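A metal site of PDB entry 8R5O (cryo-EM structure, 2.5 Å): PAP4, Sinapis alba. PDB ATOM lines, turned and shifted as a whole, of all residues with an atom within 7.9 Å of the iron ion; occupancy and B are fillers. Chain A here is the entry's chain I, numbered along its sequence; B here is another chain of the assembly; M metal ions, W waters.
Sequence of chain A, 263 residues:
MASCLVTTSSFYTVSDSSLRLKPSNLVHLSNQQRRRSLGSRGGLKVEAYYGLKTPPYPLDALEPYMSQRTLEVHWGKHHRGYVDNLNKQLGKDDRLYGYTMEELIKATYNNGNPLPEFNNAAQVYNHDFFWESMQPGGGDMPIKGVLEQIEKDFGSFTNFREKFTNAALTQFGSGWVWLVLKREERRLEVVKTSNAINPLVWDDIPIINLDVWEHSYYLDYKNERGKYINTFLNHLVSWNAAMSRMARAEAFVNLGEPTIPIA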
ATOM      1  N   HIS A  74      31.484 -15.544   2.383  1.00  0.00           N
ATOM      2  CA  HIS A  74      30.601 -14.641   1.642  1.00  0.00           C
ATOM      3  C   HIS A  74      30.965 -14.606   0.165  1.00  0.00           C
ATOM      4  O   HIS A  74      30.088 -14.710  -0.702  1.00  0.00           O
ATOM      5  CB  HIS A  74      30.661 -13.241   2.249  1.00  0.00           C
ATOM      6  CG  HIS A  74      29.502 -12.368   1.870  1.00  0.00           C
ATOM      7  ND1 HIS A  74      29.320 -11.111   2.394  1.00  0.00           N
ATOM      8  CD2 HIS A  74      28.471 -12.573   1.021  1.00  0.00           C
ATOM      9  CE1 HIS A  74      28.222 -10.570   1.880  1.00  0.00           C
ATOM     10  NE2 HIS A  74      27.689 -11.444   1.045  1.00  0.00           N
ATOM     11  N   TRP A  75      32.254 -14.456  -0.149  1.00  0.00           N
ATOM     12  CA  TRP A  75      32.668 -14.427  -1.548  1.00  0.00           C
ATOM     13  C   TRP A  75      32.903 -15.831  -2.093  1.00  0.00           C
ATOM     14  O   TRP A  75      32.457 -16.157  -3.198  1.00  0.00           O
ATOM     15  CB  TRP A  75      33.937 -13.573  -1.698  1.00  0.00           C
ATOM     16  CG  TRP A  75      34.470 -13.557  -3.101  1.00  0.00           C
ATOM     17  CD1 TRP A  75      34.068 -12.757  -4.123  1.00  0.00           C
ATOM     18  CD2 TRP A  75      35.523 -14.390  -3.622  1.00  0.00           C
ATOM     19  NE1 TRP A  75      34.795 -13.039  -5.250  1.00  0.00           N
ATOM     20  CE2 TRP A  75      35.699 -14.031  -4.966  1.00  0.00           C
ATOM     21  CE3 TRP A  75      36.325 -15.393  -3.072  1.00  0.00           C
ATOM     22  CZ2 TRP A  75      36.638 -14.647  -5.785  1.00  0.00           C
ATOM     23  CZ3 TRP A  75      37.260 -16.001  -3.895  1.00  0.00           C
ATOM     24  CH2 TRP A  75      37.412 -15.626  -5.231  1.00  0.00           C
ATOM     25  N   HIS A  78      28.990 -18.032  -1.096  1.00  0.00           N
ATOM     26  CA  HIS A  78      27.727 -17.414  -1.510  1.00  0.00           C
ATOM     27  C   HIS A  78      27.838 -16.814  -2.904  1.00  0.00           C
ATOM     28  O   HIS A  78      27.078 -17.156  -3.814  1.00  0.00           O
ATOM     29  CB  HIS A  78      27.298 -16.357  -0.500  1.00  0.00           C
ATOM     30  CG  HIS A  78      26.797 -16.924   0.795  1.00  0.00           C
ATOM     31  ND1 HIS A  78      25.546 -17.487   0.923  1.00  0.00           N
ATOM     32  CD2 HIS A  78      27.365 -17.001   2.015  1.00  0.00           C
ATOM     33  CE1 HIS A  78      25.368 -17.889   2.168  1.00  0.00           C
ATOM     34  NE2 HIS A  78      26.466 -17.611   2.851  1.00  0.00           N
ATOM     35  N   HIS A  79      28.802 -15.909  -3.091  1.00  0.00           N
ATOM     36  CA  HIS A  79      28.964 -15.266  -4.388  1.00  0.00           C
ATOM     37  C   HIS A  79      29.327 -16.280  -5.462  1.00  0.00           C
ATOM     38  O   HIS A  79      28.814 -16.222  -6.586  1.00  0.00           O
ATOM     39  CB  HIS A  79      30.030 -14.168  -4.305  1.00  0.00           C
ATOM     40  CG  HIS A  79      30.048 -13.245  -5.483  1.00  0.00           C
ATOM     41  ND1 HIS A  79      30.934 -12.205  -5.599  1.00  0.00           N
ATOM     42  CD2 HIS A  79      29.262 -13.201  -6.587  1.00  0.00           C
ATOM     43  CE1 HIS A  79      30.710 -11.555  -6.725  1.00  0.00           C
ATOM     44  NE2 HIS A  79      29.698 -12.146  -7.349  1.00  0.00           N
ATOM     45  N   TYR A  82      26.203 -18.226  -6.544  1.00  0.00           N
ATOM     46  CA  TYR A  82      25.347 -17.453  -7.434  1.00  0.00           C
ATOM     47  C   TYR A  82      25.870 -17.470  -8.864  1.00  0.00           C
ATOM     48  O   TYR A  82      25.095 -17.613  -9.812  1.00  0.00           O
ATOM     49  CB  TYR A  82      25.233 -16.018  -6.930  1.00  0.00           C
ATOM     50  CG  TYR A  82      24.422 -15.868  -5.658  1.00  0.00           C
ATOM     51  CD1 TYR A  82      23.200 -16.513  -5.525  1.00  0.00           C
ATOM     52  CD2 TYR A  82      24.875 -15.097  -4.607  1.00  0.00           C
ATOM     53  CE1 TYR A  82      22.455 -16.378  -4.369  1.00  0.00           C
ATOM     54  CE2 TYR A  82      24.142 -14.959  -3.458  1.00  0.00           C
ATOM     55  CZ  TYR A  82      22.928 -15.594  -3.337  1.00  0.00           C
ATOM     56  OH  TYR A  82      22.199 -15.464  -2.183  1.00  0.00           O
ATOM     57  N   GLN A 123      21.820 -11.300  -7.881  1.00  0.00           N
ATOM     58  CA  GLN A 123      22.755 -11.445  -6.763  1.00  0.00           C
ATOM     59  C   GLN A 123      24.212 -11.354  -7.193  1.00  0.00           C
ATOM     60  O   GLN A 123      25.037 -10.850  -6.424  1.00  0.00           O
ATOM     61  CB  GLN A 123      22.501 -12.770  -6.030  1.00  0.00           C
ATOM     62  CG  GLN A 123      21.314 -12.736  -5.073  1.00  0.00           C
ATOM     63  CD  GLN A 123      21.549 -11.844  -3.856  1.00  0.00           C
ATOM     64  OE1 GLN A 123      21.499 -10.617  -3.956  1.00  0.00           O
ATOM     65  NE2 GLN A 123      21.795 -12.458  -2.710  1.00  0.00           N
ATOM     66  N   ASN A 126      24.842  -7.728  -7.457  1.00  0.00           N
ATOM     67  CA  ASN A 126      24.793  -7.072  -6.152  1.00  0.00           C
ATOM     68  C   ASN A 126      26.082  -7.295  -5.373  1.00  0.00           C
ATOM     69  O   ASN A 126      26.592  -6.371  -4.722  1.00  0.00           O
ATOM     70  CB  ASN A 126      23.593  -7.585  -5.344  1.00  0.00           C
ATOM     71  CG  ASN A 126      22.271  -7.144  -5.926  1.00  0.00           C
ATOM     72  OD1 ASN A 126      22.200  -6.182  -6.690  1.00  0.00           O
ATOM     73  ND2 ASN A 126      21.211  -7.857  -5.571  1.00  0.00           N
ATOM     74  N   HIS A 127      26.614  -8.519  -5.409  1.00  0.00           N
ATOM     75  CA  HIS A 127      27.829  -8.808  -4.650  1.00  0.00           C
ATOM     76  C   HIS A 127      29.059  -8.184  -5.290  1.00  0.00           C
ATOM     77  O   HIS A 127      29.933  -7.679  -4.592  1.00  0.00           O
ATOM     78  CB  HIS A 127      27.990 -10.315  -4.480  1.00  0.00           C
ATOM     79  CG  HIS A 127      27.010 -10.911  -3.512  1.00  0.00           C
ATOM     80  ND1 HIS A 127      25.739 -11.289  -3.881  1.00  0.00           N
ATOM     81  CD2 HIS A 127      27.115 -11.176  -2.189  1.00  0.00           C
ATOM     82  CE1 HIS A 127      25.107 -11.775  -2.835  1.00  0.00           C
ATOM     83  NE2 HIS A 127      25.918 -11.711  -1.790  1.00  0.00           N
ATOM     84  N   PHE A 130      28.973  -4.812  -4.280  1.00  0.00           N
ATOM     85  CA  PHE A 130      29.203  -4.653  -2.845  1.00  0.00           C
ATOM     86  C   PHE A 130      30.689  -4.689  -2.500  1.00  0.00           C
ATOM     87  O   PHE A 130      31.145  -3.899  -1.669  1.00  0.00           O
ATOM     88  CB  PHE A 130      28.451  -5.744  -2.084  1.00  0.00           C
ATOM     89  CG  PHE A 130      28.636  -5.680  -0.590  1.00  0.00           C
ATOM     90  CD1 PHE A 130      28.407  -4.508   0.102  1.00  0.00           C
ATOM     91  CD2 PHE A 130      29.027  -6.800   0.117  1.00  0.00           C
ATOM     92  CE1 PHE A 130      28.568  -4.448   1.474  1.00  0.00           C
ATOM     93  CE2 PHE A 130      29.192  -6.747   1.494  1.00  0.00           C
ATOM     94  CZ  PHE A 130      28.966  -5.574   2.164  1.00  0.00           C
ATOM     95  N   TRP A 131      31.450  -5.586  -3.117  1.00  0.00           N
ATOM     96  CA  TRP A 131      32.880  -5.653  -2.818  1.00  0.00           C
ATOM     97  C   TRP A 131      33.587  -4.369  -3.232  1.00  0.00           C
ATOM     98  O   TRP A 131      34.494  -3.896  -2.533  1.00  0.00           O
ATOM     99  CB  TRP A 131      33.530  -6.857  -3.512  1.00  0.00           C
ATOM    100  CG  TRP A 131      32.858  -8.170  -3.254  1.00  0.00           C
ATOM    101  CD1 TRP A 131      32.473  -9.095  -4.193  1.00  0.00           C
ATOM    102  CD2 TRP A 131      32.489  -8.730  -1.987  1.00  0.00           C
ATOM    103  NE1 TRP A 131      31.896 -10.171  -3.581  1.00  0.00           N
ATOM    104  CE2 TRP A 131      31.892  -9.983  -2.226  1.00  0.00           C
ATOM    105  CE3 TRP A 131      32.617  -8.294  -0.662  1.00  0.00           C
ATOM    106  CZ2 TRP A 131      31.418 -10.792  -1.212  1.00  0.00           C
ATOM    107  CZ3 TRP A 131      32.143  -9.103   0.352  1.00  0.00           C
ATOM    108  CH2 TRP A 131      31.552 -10.336   0.075  1.00  0.00           C
ATOM    109  N   GLY A 175      18.052  -8.418   2.457  1.00  0.00           N
ATOM    110  CA  GLY A 175      17.869  -7.314   1.534  1.00  0.00           C
ATOM    111  C   GLY A 175      19.156  -6.534   1.348  1.00  0.00           C
ATOM    112  O   GLY A 175      20.232  -6.969   1.730  1.00  0.00           O
ATOM    113  N   TRP A 176      18.992  -5.362   0.737  1.00  0.00           N
ATOM    114  CA  TRP A 176      20.103  -4.477   0.413  1.00  0.00           C
ATOM    115  C   TRP A 176      19.696  -3.034   0.696  1.00  0.00           C
ATOM    116  O   TRP A 176      18.508  -2.697   0.686  1.00  0.00           O
ATOM    117  CB  TRP A 176      20.551  -4.613  -1.042  1.00  0.00           C
ATOM    118  CG  TRP A 176      21.067  -5.967  -1.390  1.00  0.00           C
ATOM    119  CD1 TRP A 176      20.339  -7.081  -1.682  1.00  0.00           C
ATOM    120  CD2 TRP A 176      22.444  -6.360  -1.489  1.00  0.00           C
ATOM    121  NE1 TRP A 176      21.176  -8.134  -1.946  1.00  0.00           N
ATOM    122  CE2 TRP A 176      22.470  -7.721  -1.838  1.00  0.00           C
ATOM    123  CE3 TRP A 176      23.649  -5.681  -1.313  1.00  0.00           C
ATOM    124  CZ2 TRP A 176      23.664  -8.422  -2.009  1.00  0.00           C
ATOM    125  CZ3 TRP A 176      24.829  -6.379  -1.490  1.00  0.00           C
ATOM    126  CH2 TRP A 176      24.823  -7.730  -1.834  1.00  0.00           C
ATOM    127  N   ASP A 211      25.165  -4.783   2.044  1.00  0.00           N
ATOM    128  CA  ASP A 211      24.471  -6.061   2.158  1.00  0.00           C
ATOM    129  C   ASP A 211      23.977  -6.234   3.584  1.00  0.00           C
ATOM    130  O   ASP A 211      24.777  -6.256   4.529  1.00  0.00           O
ATOM    131  CB  ASP A 211      25.419  -7.195   1.774  1.00  0.00           C
ATOM    132  CG  ASP A 211      24.691  -8.513   1.549  1.00  0.00           C
ATOM    133  OD1 ASP A 211      23.453  -8.548   1.699  1.00  0.00           O
ATOM    134  OD2 ASP A 211      25.368  -9.510   1.226  1.00  0.00           O
ATOM    135  N   VAL A 212      22.663  -6.362   3.757  1.00  0.00           N
ATOM    136  CA  VAL A 212      22.100  -6.622   5.072  1.00  0.00           C
ATOM    137  C   VAL A 212      21.482  -8.021   5.143  1.00  0.00           C
ATOM    138  O   VAL A 212      20.684  -8.303   6.034  1.00  0.00           O
ATOM    139  CB  VAL A 212      21.093  -5.533   5.481  1.00  0.00           C
ATOM    140  CG1 VAL A 212      21.784  -4.184   5.591  1.00  0.00           C
ATOM    141  CG2 VAL A 212      19.923  -5.459   4.518  1.00  0.00           C
ATOM    142  N   TRP A 213      21.838  -8.897   4.212  1.00  0.00           N
ATOM    143  CA  TRP A 213      21.613 -10.322   4.415  1.00  0.00           C
ATOM    144  C   TRP A 213      22.375 -10.773   5.657  1.00  0.00           C
ATOM    145  O   TRP A 213      23.488 -10.311   5.923  1.00  0.00           O
ATOM    146  CB  TRP A 213      22.073 -11.131   3.200  1.00  0.00           C
ATOM    147  CG  TRP A 213      21.144 -11.090   2.028  1.00  0.00           C
ATOM    148  CD1 TRP A 213      20.753  -9.991   1.328  1.00  0.00           C
ATOM    149  CD2 TRP A 213      20.505 -12.212   1.402  1.00  0.00           C
ATOM    150  NE1 TRP A 213      19.904 -10.353   0.311  1.00  0.00           N
ATOM    151  CE2 TRP A 213      19.737 -11.706   0.332  1.00  0.00           C
ATOM    152  CE3 TRP A 213      20.507 -13.589   1.646  1.00  0.00           C
ATOM    153  CZ2 TRP A 213      18.975 -12.533  -0.485  1.00  0.00           C
ATOM    154  CZ3 TRP A 213      19.762 -14.404   0.831  1.00  0.00           C
ATOM    155  CH2 TRP A 213      18.998 -13.874  -0.223  1.00  0.00           C
ATOM    156  N   GLU A 214      21.772 -11.671   6.435  1.00  0.00           N
ATOM    157  CA  GLU A 214      22.377 -12.072   7.698  1.00  0.00           C
ATOM    158  C   GLU A 214      23.732 -12.736   7.500  1.00  0.00           C
ATOM    159  O   GLU A 214      24.590 -12.645   8.386  1.00  0.00           O
ATOM    160  CB  GLU A 214      21.425 -12.990   8.468  1.00  0.00           C
ATOM    161  CG  GLU A 214      20.347 -12.240   9.232  1.00  0.00           C
ATOM    162  CD  GLU A 214      19.380 -13.157   9.951  1.00  0.00           C
ATOM    163  OE1 GLU A 214      19.113 -14.265   9.435  1.00  0.00           O
ATOM    164  OE2 GLU A 214      18.875 -12.772  11.018  1.00  0.00           O
ATOM    165  N   HIS A 215      23.951 -13.384   6.361  1.00  0.00           N
ATOM    166  CA  HIS A 215      25.223 -14.059   6.134  1.00  0.00           C
ATOM    167  C   HIS A 215      26.395 -13.083   6.006  1.00  0.00           C
ATOM    168  O   HIS A 215      27.543 -13.527   6.092  1.00  0.00           O
ATOM    169  CB  HIS A 215      25.155 -14.960   4.896  1.00  0.00           C
ATOM    170  CG  HIS A 215      24.949 -14.238   3.606  1.00  0.00           C
ATOM    171  ND1 HIS A 215      23.874 -14.477   2.785  1.00  0.00           N
ATOM    172  CD2 HIS A 215      25.688 -13.295   2.979  1.00  0.00           C
ATOM    173  CE1 HIS A 215      23.956 -13.717   1.709  1.00  0.00           C
ATOM    174  NE2 HIS A 215      25.049 -12.977   1.809  1.00  0.00           N
ATOM    175  N   SER A 216      26.130 -11.798   5.813  1.00  0.00           N
ATOM    176  CA  SER A 216      27.197 -10.815   5.641  1.00  0.00           C
ATOM    177  C   SER A 216      27.750 -10.287   6.959  1.00  0.00           C
ATOM    178  O   SER A 216      28.841  -9.697   6.949  1.00  0.00           O
ATOM    179  CB  SER A 216      26.699  -9.641   4.795  1.00  0.00           C
ATOM    180  OG  SER A 216      25.634  -8.967   5.431  1.00  0.00           O
ATOM    181  N   TYR A 228      27.180  -3.483  12.844  1.00  0.00           N
ATOM    182  CA  TYR A 228      27.681  -3.767  11.504  1.00  0.00           C
ATOM    183  C   TYR A 228      27.468  -2.581  10.576  1.00  0.00           C
ATOM    184  O   TYR A 228      28.341  -2.250   9.766  1.00  0.00           O
ATOM    185  CB  TYR A 228      26.987  -5.012  10.965  1.00  0.00           C
ATOM    186  CG  TYR A 228      27.089  -5.219   9.475  1.00  0.00           C
ATOM    187  CD1 TYR A 228      28.304  -5.560   8.878  1.00  0.00           C
ATOM    188  CD2 TYR A 228      25.974  -5.084   8.660  1.00  0.00           C
ATOM    189  CE1 TYR A 228      28.389  -5.758   7.514  1.00  0.00           C
ATOM    190  CE2 TYR A 228      26.059  -5.283   7.296  1.00  0.00           C
ATOM    191  CZ  TYR A 228      27.272  -5.614   6.740  1.00  0.00           C
ATOM    192  OH  TYR A 228      27.358  -5.812   5.375  1.00  0.00           O
ATOM    193  N   GLU B 226      18.678 -17.398   8.025  1.00  0.00           N
ATOM    194  CA  GLU B 226      20.079 -17.804   8.109  1.00  0.00           C
ATOM    195  C   GLU B 226      20.584 -17.860   9.545  1.00  0.00           C
ATOM    196  O   GLU B 226      21.496 -18.633   9.849  1.00  0.00           O
ATOM    197  CB  GLU B 226      20.944 -16.878   7.257  1.00  0.00           C
ATOM    198  CG  GLU B 226      20.784 -17.130   5.768  1.00  0.00           C
ATOM    199  CD  GLU B 226      21.570 -16.154   4.901  1.00  0.00           C
ATOM    200  OE1 GLU B 226      21.657 -14.971   5.275  1.00  0.00           O
ATOM    201  OE2 GLU B 226      22.089 -16.584   3.854  1.00  0.00           O
HETATM  202 FE    FE M   1      25.584 -11.447   0.242  1.00  0.00          FE
HETATM  203  O   HOH W   1      23.523 -11.194  -0.121  1.00  0.00           O
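The backbone carbonyl oxygen (O) of Asp 211 sits at hydrogen-bond distance from the side-chain hydroxyl (OG) of Ser 216 (3.0 Å).
O of His 127 sits close to NE1 of Trp 131, 3.3 Å away.
ND1 of His 215 lies within hydrogen-bond range of OE2 of Glu 226 of chain B (3.0 Å).
The side-chain hydroxyl (OH) of Tyr 228 sits at hydrogen-bond distance from the backbone carbonyl oxygen (O) of Asp 211 (2.8 Å).
OD1 of Asp 211 is in hydrogen-bond range of N of Trp 213 (3.0 Å).
A ring nitrogen (ND1) of His 127 is in hydrogen-bond range of the backbone carbonyl oxygen (O) of Gln 123.
The backbone carbonyl oxygen (O) of His 74 sits at hydrogen-bond distance from the backbone NH (N) of His 79.
Of the 20 residues printed, 4 come within 4 Å of the iron ion.
The nearest printed residue that does not touch the iron ion is Trp 176 (4.2 Å).
The iron ion is bound by NE2 of His 127, water W1, OD2 of Asp 211, NE2 of His 74 and NE2 of His 215.
Water W1 lies within hydrogen-bond range of the side-chain carboxylate (OD1) of Asp 211 (3.2 Å) and the side-chain amide nitrogen (NE2) of Gln 123 (3.4 Å).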
